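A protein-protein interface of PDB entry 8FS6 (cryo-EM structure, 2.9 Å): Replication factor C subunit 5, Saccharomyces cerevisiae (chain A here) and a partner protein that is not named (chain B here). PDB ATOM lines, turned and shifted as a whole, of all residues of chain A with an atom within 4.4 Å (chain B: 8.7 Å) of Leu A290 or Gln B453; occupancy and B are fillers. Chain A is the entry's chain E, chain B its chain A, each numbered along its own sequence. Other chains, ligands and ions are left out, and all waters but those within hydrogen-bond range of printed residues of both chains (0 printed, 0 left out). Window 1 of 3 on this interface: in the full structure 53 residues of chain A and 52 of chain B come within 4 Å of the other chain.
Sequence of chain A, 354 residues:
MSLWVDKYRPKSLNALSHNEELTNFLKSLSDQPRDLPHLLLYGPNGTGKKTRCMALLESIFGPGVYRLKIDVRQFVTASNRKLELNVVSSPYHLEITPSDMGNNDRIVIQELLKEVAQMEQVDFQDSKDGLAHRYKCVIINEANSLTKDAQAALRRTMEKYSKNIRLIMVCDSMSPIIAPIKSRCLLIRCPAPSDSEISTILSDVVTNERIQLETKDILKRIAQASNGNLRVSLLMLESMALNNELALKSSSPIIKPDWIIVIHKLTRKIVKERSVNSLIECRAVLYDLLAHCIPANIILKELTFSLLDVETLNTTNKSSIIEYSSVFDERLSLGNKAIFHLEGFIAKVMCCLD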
ATOM      1  N   LEU A 286     -36.471  12.472   2.734  1.00  0.00           N
ATOM      2  CA  LEU A 286     -35.474  11.504   2.286  1.00  0.00           C
ATOM      3  C   LEU A 286     -34.639  12.054   1.139  1.00  0.00           C
ATOM      4  O   LEU A 286     -33.426  11.830   1.086  1.00  0.00           O
ATOM      5  CB  LEU A 286     -36.157  10.202   1.868  1.00  0.00           C
ATOM      6  CG  LEU A 286     -36.710   9.309   2.978  1.00  0.00           C
ATOM      7  CD1 LEU A 286     -37.507   8.169   2.373  1.00  0.00           C
ATOM      8  CD2 LEU A 286     -35.589   8.779   3.857  1.00  0.00           C
ATOM      9  N   TYR A 287     -35.272  12.759   0.199  1.00  0.00           N
ATOM     10  CA  TYR A 287     -34.533  13.380  -0.894  1.00  0.00           C
ATOM     11  C   TYR A 287     -33.600  14.464  -0.375  1.00  0.00           C
ATOM     12  O   TYR A 287     -32.475  14.614  -0.867  1.00  0.00           O
ATOM     13  CB  TYR A 287     -35.502  13.958  -1.926  1.00  0.00           C
ATOM     14  CG  TYR A 287     -35.936  12.976  -2.988  1.00  0.00           C
ATOM     15  CD1 TYR A 287     -35.025  12.106  -3.572  1.00  0.00           C
ATOM     16  CD2 TYR A 287     -37.255  12.928  -3.418  1.00  0.00           C
ATOM     17  CE1 TYR A 287     -35.418  11.208  -4.547  1.00  0.00           C
ATOM     18  CE2 TYR A 287     -37.656  12.036  -4.395  1.00  0.00           C
ATOM     19  CZ  TYR A 287     -36.735  11.178  -4.954  1.00  0.00           C
ATOM     20  OH  TYR A 287     -37.135  10.288  -5.924  1.00  0.00           O
ATOM     21  N   ASP A 288     -34.056  15.234   0.616  1.00  0.00           N
ATOM     22  CA  ASP A 288     -33.195  16.242   1.227  1.00  0.00           C
ATOM     23  C   ASP A 288     -31.982  15.596   1.889  1.00  0.00           C
ATOM     24  O   ASP A 288     -30.859  16.102   1.775  1.00  0.00           O
ATOM     25  CB  ASP A 288     -33.999  17.058   2.239  1.00  0.00           C
ATOM     26  CG  ASP A 288     -33.216  18.222   2.810  1.00  0.00           C
ATOM     27  OD1 ASP A 288     -32.173  18.594   2.232  1.00  0.00           O
ATOM     28  OD2 ASP A 288     -33.651  18.772   3.842  1.00  0.00           O
ATOM     29  N   LEU A 289     -32.192  14.478   2.588  1.00  0.00           N
ATOM     30  CA  LEU A 289     -31.075  13.763   3.200  1.00  0.00           C
ATOM     31  C   LEU A 289     -30.138  13.182   2.145  1.00  0.00           C
ATOM     32  O   LEU A 289     -28.913  13.207   2.314  1.00  0.00           O
ATOM     33  CB  LEU A 289     -31.600  12.658   4.117  1.00  0.00           C
ATOM     34  CG  LEU A 289     -32.273  13.106   5.415  1.00  0.00           C
ATOM     35  CD1 LEU A 289     -32.920  11.923   6.118  1.00  0.00           C
ATOM     36  CD2 LEU A 289     -31.272  13.795   6.329  1.00  0.00           C
ATOM     37  N   LEU A 290     -30.697  12.650   1.056  1.00  0.00           N
ATOM     38  CA  LEU A 290     -29.884  12.046   0.005  1.00  0.00           C
ATOM     39  C   LEU A 290     -29.071  13.088  -0.748  1.00  0.00           C
ATOM     40  O   LEU A 290     -27.976  12.783  -1.234  1.00  0.00           O
ATOM     41  CB  LEU A 290     -30.772  11.271  -0.967  1.00  0.00           C
ATOM     42  CG  LEU A 290     -31.245   9.887  -0.522  1.00  0.00           C
ATOM     43  CD1 LEU A 290     -32.015   9.201  -1.639  1.00  0.00           C
ATOM     44  CD2 LEU A 290     -30.064   9.037  -0.080  1.00  0.00           C
ATOM     45  N   ALA A 291     -29.582  14.316  -0.853  1.00  0.00           N
ATOM     46  CA  ALA A 291     -28.855  15.386  -1.524  1.00  0.00           C
ATOM     47  C   ALA A 291     -27.591  15.797  -0.781  1.00  0.00           C
ATOM     48  O   ALA A 291     -26.768  16.523  -1.348  1.00  0.00           O
ATOM     49  CB  ALA A 291     -29.765  16.601  -1.705  1.00  0.00           C
ATOM     50  N   HIS A 292     -27.419  15.351   0.464  1.00  0.00           N
ATOM     51  CA  HIS A 292     -26.272  15.706   1.286  1.00  0.00           C
ATOM     52  C   HIS A 292     -25.228  14.596   1.340  1.00  0.00           C
ATOM     53  O   HIS A 292     -24.388  14.589   2.248  1.00  0.00           O
ATOM     54  CB  HIS A 292     -26.743  16.069   2.693  1.00  0.00           C
ATOM     55  CG  HIS A 292     -27.331  17.441   2.790  1.00  0.00           C
ATOM     56  ND1 HIS A 292     -26.725  18.550   2.243  1.00  0.00           N
ATOM     57  CD2 HIS A 292     -28.490  17.876   3.336  1.00  0.00           C
ATOM     58  CE1 HIS A 292     -27.473  19.615   2.470  1.00  0.00           C
ATOM     59  NE2 HIS A 292     -28.550  19.233   3.133  1.00  0.00           N
ATOM     60  N   CYS A 293     -25.273  13.660   0.388  1.00  0.00           N
ATOM     61  CA  CYS A 293     -24.297  12.571   0.273  1.00  0.00           C
ATOM     62  C   CYS A 293     -24.233  11.726   1.544  1.00  0.00           C
ATOM     63  O   CYS A 293     -23.162  11.286   1.966  1.00  0.00           O
ATOM     64  CB  CYS A 293     -22.912  13.107  -0.095  1.00  0.00           C
ATOM     65  SG  CYS A 293     -22.845  13.946  -1.695  1.00  0.00           S
ATOM     66  N   ILE A 294     -25.387  11.495   2.156  1.00  0.00           N
ATOM     67  CA  ILE A 294     -25.514  10.594   3.297  1.00  0.00           C
ATOM     68  C   ILE A 294     -25.867   9.213   2.757  1.00  0.00           C
ATOM     69  O   ILE A 294     -26.857   9.089   2.019  1.00  0.00           O
ATOM     70  CB  ILE A 294     -26.573  11.086   4.295  1.00  0.00           C
ATOM     71  CG1 ILE A 294     -26.390  12.578   4.573  1.00  0.00           C
ATOM     72  CG2 ILE A 294     -26.487  10.296   5.591  1.00  0.00           C
ATOM     73  CD1 ILE A 294     -27.439  13.161   5.493  1.00  0.00           C
ATOM     74  N   ILE A 299     -28.818   5.852   6.579  1.00  0.00           N
ATOM     75  CA  ILE A 299     -30.115   6.488   6.795  1.00  0.00           C
ATOM     76  C   ILE A 299     -31.149   5.458   7.235  1.00  0.00           C
ATOM     77  O   ILE A 299     -31.924   5.696   8.169  1.00  0.00           O
ATOM     78  CB  ILE A 299     -30.565   7.231   5.523  1.00  0.00           C
ATOM     79  CG1 ILE A 299     -29.593   8.364   5.194  1.00  0.00           C
ATOM     80  CG2 ILE A 299     -31.981   7.767   5.686  1.00  0.00           C
ATOM     81  CD1 ILE A 299     -30.061   9.267   4.074  1.00  0.00           C
ATOM     82  N   GLU B 446     -35.179  13.636  -9.014  1.00  0.00           N
ATOM     83  CA  GLU B 446     -33.852  13.088  -8.774  1.00  0.00           C
ATOM     84  C   GLU B 446     -32.757  13.898  -9.457  1.00  0.00           C
ATOM     85  O   GLU B 446     -31.613  13.892  -8.985  1.00  0.00           O
ATOM     86  CB  GLU B 446     -33.793  11.642  -9.248  1.00  0.00           C
ATOM     87  CG  GLU B 446     -34.516  10.656  -8.362  1.00  0.00           C
ATOM     88  CD  GLU B 446     -33.558   9.655  -7.788  1.00  0.00           C
ATOM     89  OE1 GLU B 446     -33.679   9.308  -6.598  1.00  0.00           O
ATOM     90  OE2 GLU B 446     -32.617   9.287  -8.513  1.00  0.00           O
ATOM     91  N   TRP B 447     -33.078  14.588 -10.554  1.00  0.00           N
ATOM     92  CA  TRP B 447     -32.094  15.409 -11.244  1.00  0.00           C
ATOM     93  C   TRP B 447     -31.629  16.591 -10.403  1.00  0.00           C
ATOM     94  O   TRP B 447     -30.473  17.000 -10.527  1.00  0.00           O
ATOM     95  CB  TRP B 447     -32.656  15.900 -12.581  1.00  0.00           C
ATOM     96  CG  TRP B 447     -33.765  16.898 -12.455  1.00  0.00           C
ATOM     97  CD1 TRP B 447     -35.090  16.630 -12.267  1.00  0.00           C
ATOM     98  CD2 TRP B 447     -33.651  18.325 -12.528  1.00  0.00           C
ATOM     99  NE1 TRP B 447     -35.805  17.802 -12.208  1.00  0.00           N
ATOM    100  CE2 TRP B 447     -34.946  18.856 -12.366  1.00  0.00           C
ATOM    101  CE3 TRP B 447     -32.578  19.203 -12.709  1.00  0.00           C
ATOM    102  CZ2 TRP B 447     -35.198  20.226 -12.381  1.00  0.00           C
ATOM    103  CZ3 TRP B 447     -32.830  20.563 -12.723  1.00  0.00           C
ATOM    104  CH2 TRP B 447     -34.129  21.062 -12.560  1.00  0.00           C
ATOM    105  N   LYS B 448     -32.492  17.146  -9.553  1.00  0.00           N
ATOM    106  CA  LYS B 448     -32.064  18.179  -8.618  1.00  0.00           C
ATOM    107  C   LYS B 448     -31.270  17.605  -7.453  1.00  0.00           C
ATOM    108  O   LYS B 448     -30.318  18.244  -6.979  1.00  0.00           O
ATOM    109  CB  LYS B 448     -33.280  18.942  -8.086  1.00  0.00           C
ATOM    110  CG  LYS B 448     -33.012  20.402  -7.765  1.00  0.00           C
ATOM    111  CD  LYS B 448     -34.305  21.136  -7.451  1.00  0.00           C
ATOM    112  CE  LYS B 448     -35.119  21.380  -8.713  1.00  0.00           C
ATOM    113  NZ  LYS B 448     -36.584  21.359  -8.445  1.00  0.00           N
ATOM    114  N   VAL B 449     -31.642  16.408  -6.990  1.00  0.00           N
ATOM    115  CA  VAL B 449     -30.915  15.753  -5.907  1.00  0.00           C
ATOM    116  C   VAL B 449     -29.483  15.459  -6.330  1.00  0.00           C
ATOM    117  O   VAL B 449     -28.539  15.656  -5.556  1.00  0.00           O
ATOM    118  CB  VAL B 449     -31.653  14.474  -5.469  1.00  0.00           C
ATOM    119  CG1 VAL B 449     -30.842  13.712  -4.431  1.00  0.00           C
ATOM    120  CG2 VAL B 449     -33.031  14.818  -4.929  1.00  0.00           C
ATOM    121  N   ARG B 450     -29.297  14.989  -7.567  1.00  0.00           N
ATOM    122  CA  ARG B 450     -27.948  14.710  -8.054  1.00  0.00           C
ATOM    123  C   ARG B 450     -27.110  15.981  -8.152  1.00  0.00           C
ATOM    124  O   ARG B 450     -25.909  15.961  -7.863  1.00  0.00           O
ATOM    125  CB  ARG B 450     -28.013  14.004  -9.408  1.00  0.00           C
ATOM    126  CG  ARG B 450     -27.080  12.808  -9.517  1.00  0.00           C
ATOM    127  CD  ARG B 450     -27.755  11.532  -9.035  1.00  0.00           C
ATOM    128  NE  ARG B 450     -28.865  11.133  -9.894  1.00  0.00           N
ATOM    129  CZ  ARG B 450     -28.730  10.599 -11.101  1.00  0.00           C
ATOM    130  NH1 ARG B 450     -27.538  10.362 -11.625  1.00  0.00           N
ATOM    131  NH2 ARG B 450     -29.819  10.289 -11.798  1.00  0.00           N
ATOM    132  N   LYS B 451     -27.719  17.095  -8.567  1.00  0.00           N
ATOM    133  CA  LYS B 451     -26.973  18.349  -8.665  1.00  0.00           C
ATOM    134  C   LYS B 451     -26.580  18.866  -7.285  1.00  0.00           C
ATOM    135  O   LYS B 451     -25.457  19.353  -7.093  1.00  0.00           O
ATOM    136  CB  LYS B 451     -27.787  19.400  -9.426  1.00  0.00           C
ATOM    137  CG  LYS B 451     -27.639  19.379 -10.957  1.00  0.00           C
ATOM    138  CD  LYS B 451     -27.738  17.974 -11.534  1.00  0.00           C
ATOM    139  CE  LYS B 451     -28.015  17.960 -13.021  1.00  0.00           C
ATOM    140  NZ  LYS B 451     -27.938  16.565 -13.539  1.00  0.00           N
ATOM    141  N   LEU B 452     -27.488  18.761  -6.310  1.00  0.00           N
ATOM    142  CA  LEU B 452     -27.131  19.119  -4.938  1.00  0.00           C
ATOM    143  C   LEU B 452     -26.035  18.205  -4.402  1.00  0.00           C
ATOM    144  O   LEU B 452     -25.145  18.652  -3.668  1.00  0.00           O
ATOM    145  CB  LEU B 452     -28.367  19.070  -4.040  1.00  0.00           C
ATOM    146  CG  LEU B 452     -29.503  20.036  -4.383  1.00  0.00           C
ATOM    147  CD1 LEU B 452     -30.842  19.486  -3.913  1.00  0.00           C
ATOM    148  CD2 LEU B 452     -29.244  21.410  -3.784  1.00  0.00           C
ATOM    149  N   GLN B 453     -26.078  16.921  -4.768  1.00  0.00           N
ATOM    150  CA  GLN B 453     -25.030  15.992  -4.361  1.00  0.00           C
ATOM    151  C   GLN B 453     -23.685  16.373  -4.966  1.00  0.00           C
ATOM    152  O   GLN B 453     -22.651  16.277  -4.300  1.00  0.00           O
ATOM    153  CB  GLN B 453     -25.409  14.566  -4.763  1.00  0.00           C
ATOM    154  CG  GLN B 453     -26.356  13.883  -3.795  1.00  0.00           C
ATOM    155  CD  GLN B 453     -26.404  12.381  -3.989  1.00  0.00           C
ATOM    156  OE1 GLN B 453     -26.512  11.891  -5.113  1.00  0.00           O
ATOM    157  NE2 GLN B 453     -26.325  11.640  -2.889  1.00  0.00           N
ATOM    158  N   ASN B 454     -23.678  16.794  -6.232  1.00  0.00           N
ATOM    159  CA  ASN B 454     -22.432  17.224  -6.865  1.00  0.00           C
ATOM    160  C   ASN B 454     -21.893  18.496  -6.220  1.00  0.00           C
ATOM    161  O   ASN B 454     -20.675  18.647  -6.045  1.00  0.00           O
ATOM    162  CB  ASN B 454     -22.650  17.429  -8.364  1.00  0.00           C
ATOM    163  CG  ASN B 454     -22.693  16.121  -9.129  1.00  0.00           C
ATOM    164  OD1 ASN B 454     -22.616  15.042  -8.541  1.00  0.00           O
ATOM    165  ND2 ASN B 454     -22.815  16.211 -10.447  1.00  0.00           N
ATOM    166  N   SER B 455     -22.784  19.426  -5.864  1.00  0.00           N
ATOM    167  CA  SER B 455     -22.356  20.612  -5.127  1.00  0.00           C
ATOM    168  C   SER B 455     -21.747  20.230  -3.782  1.00  0.00           C
ATOM    169  O   SER B 455     -20.722  20.792  -3.371  1.00  0.00           O
ATOM    170  CB  SER B 455     -23.535  21.565  -4.933  1.00  0.00           C
ATOM    171  OG  SER B 455     -23.939  22.136  -6.165  1.00  0.00           O
ATOM    172  N   PHE B 456     -22.364  19.269  -3.089  1.00  0.00           N
ATOM    173  CA  PHE B 456     -21.807  18.774  -1.834  1.00  0.00           C
ATOM    174  C   PHE B 456     -20.444  18.128  -2.058  1.00  0.00           C
ATOM    175  O   PHE B 456     -19.537  18.277  -1.234  1.00  0.00           O
ATOM    176  CB  PHE B 456     -22.784  17.786  -1.189  1.00  0.00           C
ATOM    177  CG  PHE B 456     -22.400  17.354   0.206  1.00  0.00           C
ATOM    178  CD1 PHE B 456     -21.419  16.395   0.415  1.00  0.00           C
ATOM    179  CD2 PHE B 456     -23.057  17.876   1.307  1.00  0.00           C
ATOM    180  CE1 PHE B 456     -21.077  15.999   1.689  1.00  0.00           C
ATOM    181  CE2 PHE B 456     -22.720  17.476   2.588  1.00  0.00           C
ATOM    182  CZ  PHE B 456     -21.729  16.536   2.777  1.00  0.00           C
ATOM    183  N   LYS B 457     -20.290  17.392  -3.162  1.00  0.00           N
ATOM    184  CA  LYS B 457     -19.006  16.773  -3.483  1.00  0.00           C
ATOM    185  C   LYS B 457     -17.924  17.828  -3.663  1.00  0.00           C
ATOM    186  O   LYS B 457     -16.811  17.694  -3.140  1.00  0.00           O
ATOM    187  CB  LYS B 457     -19.135  15.928  -4.753  1.00  0.00           C
ATOM    188  CG  LYS B 457     -19.929  14.642  -4.601  1.00  0.00           C
ATOM    189  CD  LYS B 457     -19.119  13.555  -3.920  1.00  0.00           C
ATOM    190  CE  LYS B 457     -19.893  12.247  -3.876  1.00  0.00           C
ATOM    191  NZ  LYS B 457     -21.284  12.442  -3.380  1.00  0.00           N
ATOM    192  N   VAL B 458     -18.242  18.894  -4.402  1.00  0.00           N
ATOM    193  CA  VAL B 458     -17.271  19.964  -4.626  1.00  0.00           C
ATOM    194  C   VAL B 458     -16.923  20.658  -3.312  1.00  0.00           C
ATOM    195  O   VAL B 458     -15.748  20.938  -3.033  1.00  0.00           O
ATOM    196  CB  VAL B 458     -17.808  20.952  -5.679  1.00  0.00           C
ATOM    197  CG1 VAL B 458     -17.225  22.345  -5.473  1.00  0.00           C
ATOM    198  CG2 VAL B 458     -17.505  20.447  -7.082  1.00  0.00           C
ATOM    199  N   GLN B 459     -17.932  20.935  -2.480  1.00  0.00           N
ATOM    200  CA  GLN B 459     -17.676  21.597  -1.203  1.00  0.00           C
ATOM    201  C   GLN B 459     -16.836  20.724  -0.276  1.00  0.00           C
ATOM    202  O   GLN B 459     -15.946  21.226   0.419  1.00  0.00           O
ATOM    203  CB  GLN B 459     -18.996  21.981  -0.535  1.00  0.00           C
ATOM    204  CG  GLN B 459     -19.781  23.056  -1.275  1.00  0.00           C
ATOM    205  CD  GLN B 459     -18.914  24.216  -1.727  1.00  0.00           C
ATOM    206  OE1 GLN B 459     -18.176  24.804  -0.935  1.00  0.00           O
ATOM    207  NE2 GLN B 459     -18.999  24.553  -3.010  1.00  0.00           N
ATOM    208  N   ALA B 460     -17.100  19.415  -0.253  1.00  0.00           N
ATOM    209  CA  ALA B 460     -16.309  18.514   0.581  1.00  0.00           C
ATOM    210  C   ALA B 460     -14.883  18.386   0.060  1.00  0.00           C
ATOM    211  O   ALA B 460     -13.937  18.266   0.848  1.00  0.00           O
ATOM    212  CB  ALA B 460     -16.981  17.143   0.655  1.00  0.00           C
ATOM    213  N   PHE B 477     -14.149  10.929   2.922  1.00  0.00           N
ATOM    214  CA  PHE B 477     -15.367  11.608   2.492  1.00  0.00           C
ATOM    215  C   PHE B 477     -16.561  11.211   3.352  1.00  0.00           C
ATOM    216  O   PHE B 477     -17.368  12.066   3.733  1.00  0.00           O
ATOM    217  CB  PHE B 477     -15.644  11.307   1.020  1.00  0.00           C
ATOM    218  CG  PHE B 477     -16.922  11.910   0.511  1.00  0.00           C
ATOM    219  CD1 PHE B 477     -17.059  13.282   0.394  1.00  0.00           C
ATOM    220  CD2 PHE B 477     -17.990  11.102   0.153  1.00  0.00           C
ATOM    221  CE1 PHE B 477     -18.233  13.840  -0.073  1.00  0.00           C
ATOM    222  CE2 PHE B 477     -19.167  11.653  -0.315  1.00  0.00           C
ATOM    223  CZ  PHE B 477     -19.290  13.024  -0.427  1.00  0.00           C
ATOM    224  N   THR B 481     -19.135  13.691   5.423  1.00  0.00           N
ATOM    225  CA  THR B 481     -20.591  13.790   5.334  1.00  0.00           C
ATOM    226  C   THR B 481     -21.287  13.425   6.637  1.00  0.00           C
ATOM    227  O   THR B 481     -22.378  13.940   6.902  1.00  0.00           O
ATOM    228  CB  THR B 481     -21.147  12.895   4.222  1.00  0.00           C
ATOM    229  OG1 THR B 481     -21.300  11.555   4.710  1.00  0.00           O
ATOM    230  CG2 THR B 481     -20.246  12.896   3.007  1.00  0.00           C
ATOM    231  N   ILE B 539     -21.671  22.021   5.015  1.00  0.00           N
ATOM    232  CA  ILE B 539     -21.291  21.589   3.676  1.00  0.00           C
ATOM    233  C   ILE B 539     -22.540  21.273   2.869  1.00  0.00           C
ATOM    234  O   ILE B 539     -23.386  20.472   3.284  1.00  0.00           O
ATOM    235  CB  ILE B 539     -20.350  20.377   3.754  1.00  0.00           C
ATOM    236  CG1 ILE B 539     -19.057  20.751   4.481  1.00  0.00           C
ATOM    237  CG2 ILE B 539     -20.039  19.853   2.361  1.00  0.00           C
ATOM    238  CD1 ILE B 539     -18.342  21.944   3.885  1.00  0.00           C
ATOM    239  N   GLY B 540     -22.662  21.910   1.709  1.00  0.00           N
ATOM    240  CA  GLY B 540     -23.833  21.717   0.869  1.00  0.00           C
ATOM    241  C   GLY B 540     -25.094  22.328   1.440  1.00  0.00           C
ATOM    242  O   GLY B 540     -26.200  21.975   1.015  1.00  0.00           O
ATOM    243  N   ILE B 543     -29.726  21.308   6.628  1.00  0.00           N
ATOM    244  CA  ILE B 543     -30.677  20.246   6.319  1.00  0.00           C
ATOM    245  C   ILE B 543     -32.050  20.904   6.203  1.00  0.00           C
ATOM    246  O   ILE B 543     -33.083  20.225   6.162  1.00  0.00           O
ATOM    247  CB  ILE B 543     -30.664  19.144   7.397  1.00  0.00           C
ATOM    248  CG1 ILE B 543     -29.235  18.770   7.794  1.00  0.00           C
ATOM    249  CG2 ILE B 543     -31.279  17.861   6.857  1.00  0.00           C
ATOM    250  CD1 ILE B 543     -28.307  18.447   6.649  1.00  0.00           C
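The side-chain carboxylate of Asp A288 sits close to the backbone carbonyl oxygen of Ile B543. The side-chain amino group (NZ) of Lys B457 lies within hydrogen-bond range of the side-chain sulfur (SG) of Cys A293, at 2.7 Å. The side-chain amide nitrogen of Gln B453 is in hydrogen-bond range of the backbone carbonyl oxygen of Leu A290 (2.6 Å). OG1 of Thr B481 sits at hydrogen-bond distance from O of Cys A293, 3.3 Å away. The backbone carbonyl oxygen of Gln B453 is in hydrogen-bond range of the side-chain sulfur of Cys A293, at 3.5 Å.
CE1 of Tyr A287 touches OE1 of Glu B446, at 3.3 Å. CD1 of Tyr A287 touches CG2 of Val B449, 3.6 Å away. N of Ala A291 touches CG1 of Val B449, at 3.8 Å. Ala A291 touches Leu B452 (O to O, 3.5 Å). N of Gln B453 touches O of Ala A291, at 3.5 Å. Phe B456 touches His A292 (CZ to O, 3.3 Å). His A292 touches Ile B539 (ND1 to O, 3.99 Å). Gly B540 touches His A292 (O to CE1, 3.1 Å). SG of Cys A293 touches CD1 of Phe B456 (3.5 Å). CB of Cys A293 touches CZ of Phe B477, at 3.6 Å.
Printed residues of chain B within 4 Å of Cys A293: Gln B453 (3.5 Å), Phe B456 (3.5 Å), Lys B457 (2.7 Å), Phe B477 (3.6 Å) and Thr B481 (3.3 Å). Ile A299 touches none of the printed residues of chain B. Printed residues of chain A within 4 Å of Glu B446: Tyr A287 (3.3 Å). Printed residues of chain A within 4 Å of Val B449: Tyr A287 and Ala A291. Of the printed residues of chain A, Leu B452 touches Ala A291. Gln B453 touches three residues of chain A. The nearest residue of chain B that does not touch Leu A290 is Val B449 (4.1 Å).
Of the 10 printed residues of chain A, 6 touch a printed residue of chain B. Printed residues of chain A that touch a printed residue of chain B: Tyr A287, Asp A288, Leu A290, Ala A291, His A292 and Cys A293. Among the printed residues, 16 pairs touch across the chains. Among the printed residues, no Asp or Glu carboxylate lies within 4 Å of a Lys or Arg side-chain nitrogen of the other chain.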
